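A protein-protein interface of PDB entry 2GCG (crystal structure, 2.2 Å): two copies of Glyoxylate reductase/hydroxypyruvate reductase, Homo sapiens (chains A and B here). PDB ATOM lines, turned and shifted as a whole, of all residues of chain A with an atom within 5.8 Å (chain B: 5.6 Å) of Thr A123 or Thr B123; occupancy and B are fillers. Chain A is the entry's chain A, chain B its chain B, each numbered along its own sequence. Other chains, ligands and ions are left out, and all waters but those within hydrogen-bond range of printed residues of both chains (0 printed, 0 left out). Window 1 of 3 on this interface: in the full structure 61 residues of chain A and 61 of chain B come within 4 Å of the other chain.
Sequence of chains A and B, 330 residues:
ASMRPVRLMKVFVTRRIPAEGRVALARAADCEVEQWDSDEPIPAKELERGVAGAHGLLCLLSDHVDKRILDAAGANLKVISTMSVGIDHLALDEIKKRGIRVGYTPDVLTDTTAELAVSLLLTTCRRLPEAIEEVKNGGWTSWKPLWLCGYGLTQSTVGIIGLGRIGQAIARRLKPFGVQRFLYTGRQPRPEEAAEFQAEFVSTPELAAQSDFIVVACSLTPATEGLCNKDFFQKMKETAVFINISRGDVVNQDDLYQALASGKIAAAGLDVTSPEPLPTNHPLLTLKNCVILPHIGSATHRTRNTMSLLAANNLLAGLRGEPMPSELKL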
ATOM      1  N   VAL A 118     -14.338   7.071 -18.356  1.00  0.00           N
ATOM      2  CA  VAL A 118     -13.763   5.846 -17.800  1.00  0.00           C
ATOM      3  C   VAL A 118     -12.407   5.549 -18.488  1.00  0.00           C
ATOM      4  O   VAL A 118     -11.437   5.254 -17.794  1.00  0.00           O
ATOM      5  CB  VAL A 118     -14.803   4.694 -17.743  1.00  0.00           C
ATOM      6  CG1 VAL A 118     -14.197   3.434 -17.256  1.00  0.00           C
ATOM      7  CG2 VAL A 118     -15.966   5.109 -16.821  1.00  0.00           C
ATOM      8  N   SER A 119     -12.302   5.719 -19.818  1.00  0.00           N
ATOM      9  CA  SER A 119     -10.992   5.633 -20.469  1.00  0.00           C
ATOM     10  C   SER A 119      -9.973   6.479 -19.739  1.00  0.00           C
ATOM     11  O   SER A 119      -8.950   5.975 -19.358  1.00  0.00           O
ATOM     12  CB  SER A 119     -11.000   6.125 -21.906  1.00  0.00           C
ATOM     13  OG  SER A 119     -11.926   5.390 -22.656  1.00  0.00           O
ATOM     14  N   LEU A 120     -10.265   7.763 -19.541  1.00  0.00           N
ATOM     15  CA  LEU A 120      -9.317   8.643 -18.897  1.00  0.00           C
ATOM     16  C   LEU A 120      -9.037   8.241 -17.455  1.00  0.00           C
ATOM     17  O   LEU A 120      -7.917   8.291 -17.023  1.00  0.00           O
ATOM     18  CB  LEU A 120      -9.842  10.085 -18.934  1.00  0.00           C
ATOM     19  CG  LEU A 120      -9.093  11.156 -18.138  1.00  0.00           C
ATOM     20  CD1 LEU A 120      -7.720  11.273 -18.754  1.00  0.00           C
ATOM     21  CD2 LEU A 120      -9.854  12.500 -18.231  1.00  0.00           C
ATOM     22  N   LEU A 121     -10.071   7.886 -16.695  1.00  0.00           N
ATOM     23  CA  LEU A 121      -9.850   7.497 -15.313  1.00  0.00           C
ATOM     24  C   LEU A 121      -8.849   6.304 -15.238  1.00  0.00           C
ATOM     25  O   LEU A 121      -7.962   6.266 -14.377  1.00  0.00           O
ATOM     26  CB  LEU A 121     -11.193   7.193 -14.622  1.00  0.00           C
ATOM     27  CG  LEU A 121     -11.206   6.665 -13.192  1.00  0.00           C
ATOM     28  CD1 LEU A 121     -10.190   7.355 -12.329  1.00  0.00           C
ATOM     29  CD2 LEU A 121     -12.587   6.872 -12.553  1.00  0.00           C
ATOM     30  N   LEU A 122      -9.013   5.358 -16.149  1.00  0.00           N
ATOM     31  CA  LEU A 122      -8.228   4.127 -16.168  1.00  0.00           C
ATOM     32  C   LEU A 122      -6.756   4.306 -16.698  1.00  0.00           C
ATOM     33  O   LEU A 122      -5.798   3.749 -16.113  1.00  0.00           O
ATOM     34  CB  LEU A 122      -9.000   3.088 -16.983  1.00  0.00           C
ATOM     35  CG  LEU A 122      -9.699   1.764 -16.512  1.00  0.00           C
ATOM     36  CD1 LEU A 122      -9.921   1.516 -15.020  1.00  0.00           C
ATOM     37  CD2 LEU A 122     -10.976   1.614 -17.287  1.00  0.00           C
ATOM     38  N   THR A 123      -6.561   5.109 -17.751  1.00  0.00           N
ATOM     39  CA  THR A 123      -5.176   5.374 -18.202  1.00  0.00           C
ATOM     40  C   THR A 123      -4.372   6.114 -17.130  1.00  0.00           C
ATOM     41  O   THR A 123      -3.213   5.881 -16.989  1.00  0.00           O
ATOM     42  CB  THR A 123      -5.046   6.121 -19.579  1.00  0.00           C
ATOM     43  OG1 THR A 123      -5.116   7.518 -19.352  1.00  0.00           O
ATOM     44  CG2 THR A 123      -6.158   5.783 -20.545  1.00  0.00           C
ATOM     45  N   THR A 124      -5.027   7.015 -16.402  1.00  0.00           N
ATOM     46  CA  THR A 124      -4.462   7.787 -15.292  1.00  0.00           C
ATOM     47  C   THR A 124      -4.199   6.862 -14.110  1.00  0.00           C
ATOM     48  O   THR A 124      -3.082   6.790 -13.617  1.00  0.00           O
ATOM     49  CB  THR A 124      -5.486   8.927 -14.822  1.00  0.00           C
ATOM     50  OG1 THR A 124      -5.871   9.736 -15.944  1.00  0.00           O
ATOM     51  CG2 THR A 124      -4.888   9.798 -13.723  1.00  0.00           C
ATOM     52  N   CYS A 125      -5.237   6.120 -13.699  1.00  0.00           N
ATOM     53  CA  CYS A 125      -5.123   5.325 -12.522  1.00  0.00           C
ATOM     54  C   CYS A 125      -4.251   4.134 -12.741  1.00  0.00           C
ATOM     55  O   CYS A 125      -3.550   3.737 -11.809  1.00  0.00           O
ATOM     56  CB  CYS A 125      -6.481   4.963 -11.924  1.00  0.00           C
ATOM     57  SG  CYS A 125      -7.261   3.508 -12.590  1.00  0.00           S
ATOM     58  N   ARG A 126      -4.239   3.561 -13.950  1.00  0.00           N
ATOM     59  CA  ARG A 126      -3.269   2.483 -14.198  1.00  0.00           C
ATOM     60  C   ARG A 126      -1.951   2.943 -14.857  1.00  0.00           C
ATOM     61  O   ARG A 126      -1.090   2.114 -15.149  1.00  0.00           O
ATOM     62  CB  ARG A 126      -3.909   1.269 -14.880  1.00  0.00           C
ATOM     63  CG  ARG A 126      -4.995   0.549 -13.984  1.00  0.00           C
ATOM     64  CD  ARG A 126      -4.387  -0.177 -12.735  1.00  0.00           C
ATOM     65  NE  ARG A 126      -3.345  -1.114 -13.137  1.00  0.00           N
ATOM     66  CZ  ARG A 126      -3.570  -2.366 -13.510  1.00  0.00           C
ATOM     67  NH1 ARG A 126      -2.577  -3.115 -13.912  1.00  0.00           N
ATOM     68  NH2 ARG A 126      -4.783  -2.874 -13.471  1.00  0.00           N
ATOM     69  N   ARG A 127      -1.784   4.263 -15.057  1.00  0.00           N
ATOM     70  CA  ARG A 127      -0.458   4.876 -15.310  1.00  0.00           C
ATOM     71  C   ARG A 127       0.071   4.579 -16.721  1.00  0.00           C
ATOM     72  O   ARG A 127       1.288   4.595 -16.980  1.00  0.00           O
ATOM     73  CB  ARG A 127       0.574   4.430 -14.243  1.00  0.00           C
ATOM     74  CG  ARG A 127       0.297   4.928 -12.823  1.00  0.00           C
ATOM     75  CD  ARG A 127       1.305   4.412 -11.782  1.00  0.00           C
ATOM     76  NE  ARG A 127       2.623   5.028 -11.925  1.00  0.00           N
ATOM     77  CZ  ARG A 127       3.680   4.743 -11.174  1.00  0.00           C
ATOM     78  NH1 ARG A 127       3.601   3.833 -10.235  1.00  0.00           N
ATOM     79  NH2 ARG A 127       4.830   5.355 -11.386  1.00  0.00           N
ATOM     80  N   LEU A 128      -0.854   4.325 -17.636  1.00  0.00           N
ATOM     81  CA  LEU A 128      -0.533   3.992 -19.017  1.00  0.00           C
ATOM     82  C   LEU A 128       0.448   4.955 -19.720  1.00  0.00           C
ATOM     83  O   LEU A 128       1.423   4.491 -20.367  1.00  0.00           O
ATOM     84  CB  LEU A 128      -1.831   3.792 -19.809  1.00  0.00           C
ATOM     85  CG  LEU A 128      -2.483   2.378 -19.788  1.00  0.00           C
ATOM     86  CD1 LEU A 128      -2.740   1.882 -18.417  1.00  0.00           C
ATOM     87  CD2 LEU A 128      -3.764   2.306 -20.594  1.00  0.00           C
ATOM     88  N   PRO A 129       0.250   6.295 -19.593  1.00  0.00           N
ATOM     89  CA  PRO A 129       1.232   7.157 -20.317  1.00  0.00           C
ATOM     90  C   PRO A 129       2.696   7.040 -19.851  1.00  0.00           C
ATOM     91  O   PRO A 129       3.582   7.056 -20.675  1.00  0.00           O
ATOM     92  CB  PRO A 129       0.714   8.586 -20.084  1.00  0.00           C
ATOM     93  CG  PRO A 129      -0.718   8.409 -19.593  1.00  0.00           C
ATOM     94  CD  PRO A 129      -0.741   7.096 -18.856  1.00  0.00           C
ATOM     95  N   ILE A 132       3.825   3.434 -21.312  1.00  0.00           N
ATOM     96  CA  ILE A 132       4.153   3.734 -22.707  1.00  0.00           C
ATOM     97  C   ILE A 132       5.543   4.372 -22.922  1.00  0.00           C
ATOM     98  O   ILE A 132       6.323   3.928 -23.756  1.00  0.00           O
ATOM     99  CB  ILE A 132       3.020   4.628 -23.296  1.00  0.00           C
ATOM    100  CG1 ILE A 132       1.729   3.789 -23.456  1.00  0.00           C
ATOM    101  CG2 ILE A 132       3.377   5.199 -24.663  1.00  0.00           C
ATOM    102  CD1 ILE A 132       0.451   4.660 -23.677  1.00  0.00           C
ATOM    103  N   VAL A 291      -2.736  13.537 -16.531  1.00  0.00           N
ATOM    104  CA  VAL A 291      -3.067  13.257 -17.940  1.00  0.00           C
ATOM    105  C   VAL A 291      -4.023  14.312 -18.445  1.00  0.00           C
ATOM    106  O   VAL A 291      -5.043  14.617 -17.812  1.00  0.00           O
ATOM    107  CB  VAL A 291      -3.666  11.802 -18.196  1.00  0.00           C
ATOM    108  CG1 VAL A 291      -3.946  11.575 -19.699  1.00  0.00           C
ATOM    109  CG2 VAL A 291      -2.755  10.716 -17.658  1.00  0.00           C
ATOM    110  N   VAL B 118      -8.973  -3.773 -20.171  1.00  0.00           N
ATOM    111  CA  VAL B 118      -9.997  -2.836 -20.603  1.00  0.00           C
ATOM    112  C   VAL B 118      -9.381  -1.450 -20.611  1.00  0.00           C
ATOM    113  O   VAL B 118      -9.783  -0.601 -21.423  1.00  0.00           O
ATOM    114  CB  VAL B 118     -11.271  -2.837 -19.670  1.00  0.00           C
ATOM    115  CG1 VAL B 118     -12.346  -1.855 -20.186  1.00  0.00           C
ATOM    116  CG2 VAL B 118     -11.888  -4.253 -19.571  1.00  0.00           C
ATOM    117  N   SER B 119      -8.437  -1.191 -19.686  1.00  0.00           N
ATOM    118  CA  SER B 119      -7.703   0.075 -19.711  1.00  0.00           C
ATOM    119  C   SER B 119      -7.071   0.291 -21.101  1.00  0.00           C
ATOM    120  O   SER B 119      -7.239   1.379 -21.716  1.00  0.00           O
ATOM    121  CB  SER B 119      -6.598   0.117 -18.628  1.00  0.00           C
ATOM    122  OG  SER B 119      -7.153   0.168 -17.309  1.00  0.00           O
ATOM    123  N   LEU B 120      -6.362  -0.764 -21.564  1.00  0.00           N
ATOM    124  CA  LEU B 120      -5.589  -0.784 -22.816  1.00  0.00           C
ATOM    125  C   LEU B 120      -6.513  -0.678 -23.996  1.00  0.00           C
ATOM    126  O   LEU B 120      -6.218   0.005 -24.952  1.00  0.00           O
ATOM    127  CB  LEU B 120      -4.840  -2.109 -22.958  1.00  0.00           C
ATOM    128  CG  LEU B 120      -3.487  -2.265 -23.640  1.00  0.00           C
ATOM    129  CD1 LEU B 120      -3.188  -3.736 -23.968  1.00  0.00           C
ATOM    130  CD2 LEU B 120      -3.083  -1.295 -24.776  1.00  0.00           C
ATOM    131  N   LEU B 121      -7.626  -1.391 -23.937  1.00  0.00           N
ATOM    132  CA  LEU B 121      -8.594  -1.355 -25.050  1.00  0.00           C
ATOM    133  C   LEU B 121      -9.175   0.037 -25.209  1.00  0.00           C
ATOM    134  O   LEU B 121      -9.266   0.591 -26.319  1.00  0.00           O
ATOM    135  CB  LEU B 121      -9.675  -2.442 -24.839  1.00  0.00           C
ATOM    136  CG  LEU B 121     -11.175  -2.435 -25.218  1.00  0.00           C
ATOM    137  CD1 LEU B 121     -11.787  -1.210 -25.904  1.00  0.00           C
ATOM    138  CD2 LEU B 121     -11.589  -3.715 -25.904  1.00  0.00           C
ATOM    139  N   LEU B 122      -9.563   0.624 -24.083  1.00  0.00           N
ATOM    140  CA  LEU B 122     -10.033   2.001 -24.100  1.00  0.00           C
ATOM    141  C   LEU B 122      -8.941   3.037 -24.451  1.00  0.00           C
ATOM    142  O   LEU B 122      -9.212   3.973 -25.219  1.00  0.00           O
ATOM    143  CB  LEU B 122     -10.744   2.343 -22.787  1.00  0.00           C
ATOM    144  CG  LEU B 122     -12.047   1.615 -22.430  1.00  0.00           C
ATOM    145  CD1 LEU B 122     -12.408   2.044 -21.072  1.00  0.00           C
ATOM    146  CD2 LEU B 122     -13.163   1.989 -23.412  1.00  0.00           C
ATOM    147  N   THR B 123      -7.716   2.902 -23.934  1.00  0.00           N
ATOM    148  CA  THR B 123      -6.692   3.889 -24.331  1.00  0.00           C
ATOM    149  C   THR B 123      -6.497   3.821 -25.853  1.00  0.00           C
ATOM    150  O   THR B 123      -6.420   4.835 -26.521  1.00  0.00           O
ATOM    151  CB  THR B 123      -5.303   3.737 -23.597  1.00  0.00           C
ATOM    152  OG1 THR B 123      -4.765   5.038 -23.284  1.00  0.00           O
ATOM    153  CG2 THR B 123      -4.316   3.084 -24.492  1.00  0.00           C
ATOM    154  N   THR B 124      -6.455   2.604 -26.380  1.00  0.00           N
ATOM    155  CA  THR B 124      -6.232   2.353 -27.789  1.00  0.00           C
ATOM    156  C   THR B 124      -7.417   2.832 -28.654  1.00  0.00           C
ATOM    157  O   THR B 124      -7.228   3.496 -29.655  1.00  0.00           O
ATOM    158  CB  THR B 124      -5.938   0.828 -28.030  1.00  0.00           C
ATOM    159  OG1 THR B 124      -4.924   0.355 -27.124  1.00  0.00           O
ATOM    160  CG2 THR B 124      -5.487   0.530 -29.474  1.00  0.00           C
ATOM    161  N   CYS B 125      -8.637   2.484 -28.287  1.00  0.00           N
ATOM    162  CA  CYS B 125      -9.744   2.670 -29.232  1.00  0.00           C
ATOM    163  C   CYS B 125     -10.238   4.120 -29.203  1.00  0.00           C
ATOM    164  O   CYS B 125     -10.708   4.623 -30.224  1.00  0.00           O
ATOM    165  CB  CYS B 125     -10.874   1.672 -28.992  1.00  0.00           C
ATOM    166  SG  CYS B 125     -11.982   2.070 -27.601  1.00  0.00           S
ATOM    167  N   ARG B 126     -10.103   4.788 -28.045  1.00  0.00           N
ATOM    168  CA  ARG B 126     -10.378   6.234 -27.950  1.00  0.00           C
ATOM    169  C   ARG B 126      -9.145   7.182 -28.201  1.00  0.00           C
ATOM    170  O   ARG B 126      -9.224   8.429 -28.070  1.00  0.00           O
ATOM    171  CB  ARG B 126     -11.143   6.532 -26.655  1.00  0.00           C
ATOM    172  CG  ARG B 126     -12.535   5.821 -26.581  1.00  0.00           C
ATOM    173  CD  ARG B 126     -13.489   6.243 -27.754  1.00  0.00           C
ATOM    174  NE  ARG B 126     -13.522   7.709 -27.828  1.00  0.00           N
ATOM    175  CZ  ARG B 126     -14.346   8.473 -27.123  1.00  0.00           C
ATOM    176  NH1 ARG B 126     -15.272   7.906 -26.335  1.00  0.00           N
ATOM    177  NH2 ARG B 126     -14.259   9.803 -27.235  1.00  0.00           N
ATOM    178  N   ARG B 127      -8.020   6.570 -28.550  1.00  0.00           N
ATOM    179  CA  ARG B 127      -6.827   7.269 -29.122  1.00  0.00           C
ATOM    180  C   ARG B 127      -6.130   8.213 -28.178  1.00  0.00           C
ATOM    181  O   ARG B 127      -5.638   9.249 -28.584  1.00  0.00           O
ATOM    182  CB  ARG B 127      -7.173   7.966 -30.426  1.00  0.00           C
ATOM    183  CG  ARG B 127      -7.758   6.968 -31.424  1.00  0.00           C
ATOM    184  CD  ARG B 127      -8.310   7.728 -32.607  1.00  0.00           C
ATOM    185  NE  ARG B 127      -7.226   8.314 -33.396  1.00  0.00           N
ATOM    186  CZ  ARG B 127      -7.417   9.128 -34.419  1.00  0.00           C
ATOM    187  NH1 ARG B 127      -8.661   9.433 -34.747  1.00  0.00           N
ATOM    188  NH2 ARG B 127      -6.357   9.593 -35.121  1.00  0.00           N
ATOM    189  N   LEU B 128      -6.076   7.815 -26.914  1.00  0.00           N
ATOM    190  CA  LEU B 128      -5.599   8.661 -25.859  1.00  0.00           C
ATOM    191  C   LEU B 128      -4.167   9.109 -26.011  1.00  0.00           C
ATOM    192  O   LEU B 128      -3.896  10.283 -25.849  1.00  0.00           O
ATOM    193  CB  LEU B 128      -5.926   8.076 -24.503  1.00  0.00           C
ATOM    194  CG  LEU B 128      -7.339   8.379 -23.947  1.00  0.00           C
ATOM    195  CD1 LEU B 128      -8.478   7.826 -24.759  1.00  0.00           C
ATOM    196  CD2 LEU B 128      -7.433   7.857 -22.541  1.00  0.00           C
ATOM    197  N   PRO B 129      -3.254   8.196 -26.373  1.00  0.00           N
ATOM    198  CA  PRO B 129      -1.867   8.594 -26.700  1.00  0.00           C
ATOM    199  C   PRO B 129      -1.716   9.707 -27.732  1.00  0.00           C
ATOM    200  O   PRO B 129      -1.085  10.715 -27.442  1.00  0.00           O
ATOM    201  CB  PRO B 129      -1.235   7.287 -27.231  1.00  0.00           C
ATOM    202  CG  PRO B 129      -1.946   6.229 -26.493  1.00  0.00           C
ATOM    203  CD  PRO B 129      -3.416   6.729 -26.443  1.00  0.00           C
ATOM    204  N   ILE B 132      -3.121  12.772 -26.089  1.00  0.00           N
ATOM    205  CA  ILE B 132      -2.181  13.261 -25.104  1.00  0.00           C
ATOM    206  C   ILE B 132      -1.070  14.077 -25.795  1.00  0.00           C
ATOM    207  O   ILE B 132      -0.735  15.172 -25.351  1.00  0.00           O
ATOM    208  CB  ILE B 132      -1.549  12.157 -24.258  1.00  0.00           C
ATOM    209  CG1 ILE B 132      -2.618  11.626 -23.309  1.00  0.00           C
ATOM    210  CG2 ILE B 132      -0.229  12.743 -23.513  1.00  0.00           C
ATOM    211  CD1 ILE B 132      -2.282  10.353 -22.570  1.00  0.00           C
ATOM    212  N   VAL B 291      -0.459   0.768 -29.606  1.00  0.00           N
ATOM    213  CA  VAL B 291      -0.134   1.103 -28.232  1.00  0.00           C
ATOM    214  C   VAL B 291       0.559  -0.116 -27.601  1.00  0.00           C
ATOM    215  O   VAL B 291       0.070  -1.235 -27.745  1.00  0.00           O
ATOM    216  CB  VAL B 291      -1.391   1.495 -27.399  1.00  0.00           C
ATOM    217  CG1 VAL B 291      -1.015   1.888 -25.940  1.00  0.00           C
ATOM    218  CG2 VAL B 291      -2.167   2.623 -28.085  1.00  0.00           C
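The backbone carbonyl oxygen (O) of Thr A123 is in hydrogen-bond range of the backbone NH (N) of Leu A128, at 2.9 Å. O of Thr B123 is in hydrogen-bond range of N of Leu B128 (3.0 Å).
Among the printed residues, merely in contact across the chains: Ser A119 with Leu B122, Ser A119 with Arg B126, Ser A119 with Leu B128, Leu A122 with Ser B119, Thr A123 with Thr B123, Thr A123 with Leu B128, Arg A126 with Ser B119, Leu A128 with Ser B119, Leu A128 with Thr B123, Pro A129 with Ile B132, Ile A132 with Val B291 and Val A291 with Ile B132.
Val A118 touches none of the printed residues of chain B. Printed residues of chain B within 4 Å of Leu A122: Ser B119. Printed residues of chain B within 4 Å of Arg A126: Ser B119. Of the printed residues of chain A, Leu B122 touches Ser A119 (3.3 Å). Thr B123 touches two residues of chain A. The nearest printed residue of chain B that does not touch Ser A119 is Thr B123 (5.0 Å).
Of the 14 printed residues of chain B, 7 touch a printed residue of chain A. Of the 14 printed residues of chain A, 8 touch a printed residue of chain B. Hydrophobic or aromatic side chains of chain A within 4 Å of the printed part of chain B: Leu A122, Leu A128, Pro A129, Ile A132 and Val A291. Among the printed residues, no Asp or Glu carboxylate lies within 4 Å of a Lys or Arg side-chain nitrogen of the other chain.
Ser A119 touches Leu B122, and with the chains exchanged Leu A122 touches Ser B119. Ser A119 touches Arg B126, and with the chains exchanged Arg A126 touches Ser B119. Ser A119 touches Leu B128, and with the chains exchanged Leu A128 touches Ser B119. Thr A123 touches Leu B128, and with the chains exchanged Leu A128 touches Thr B123. Positions printed for both chains: 118, 119, 120, 121, 122, 123, 124, 125, 126, 127, 128, 129, 132 and 291.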
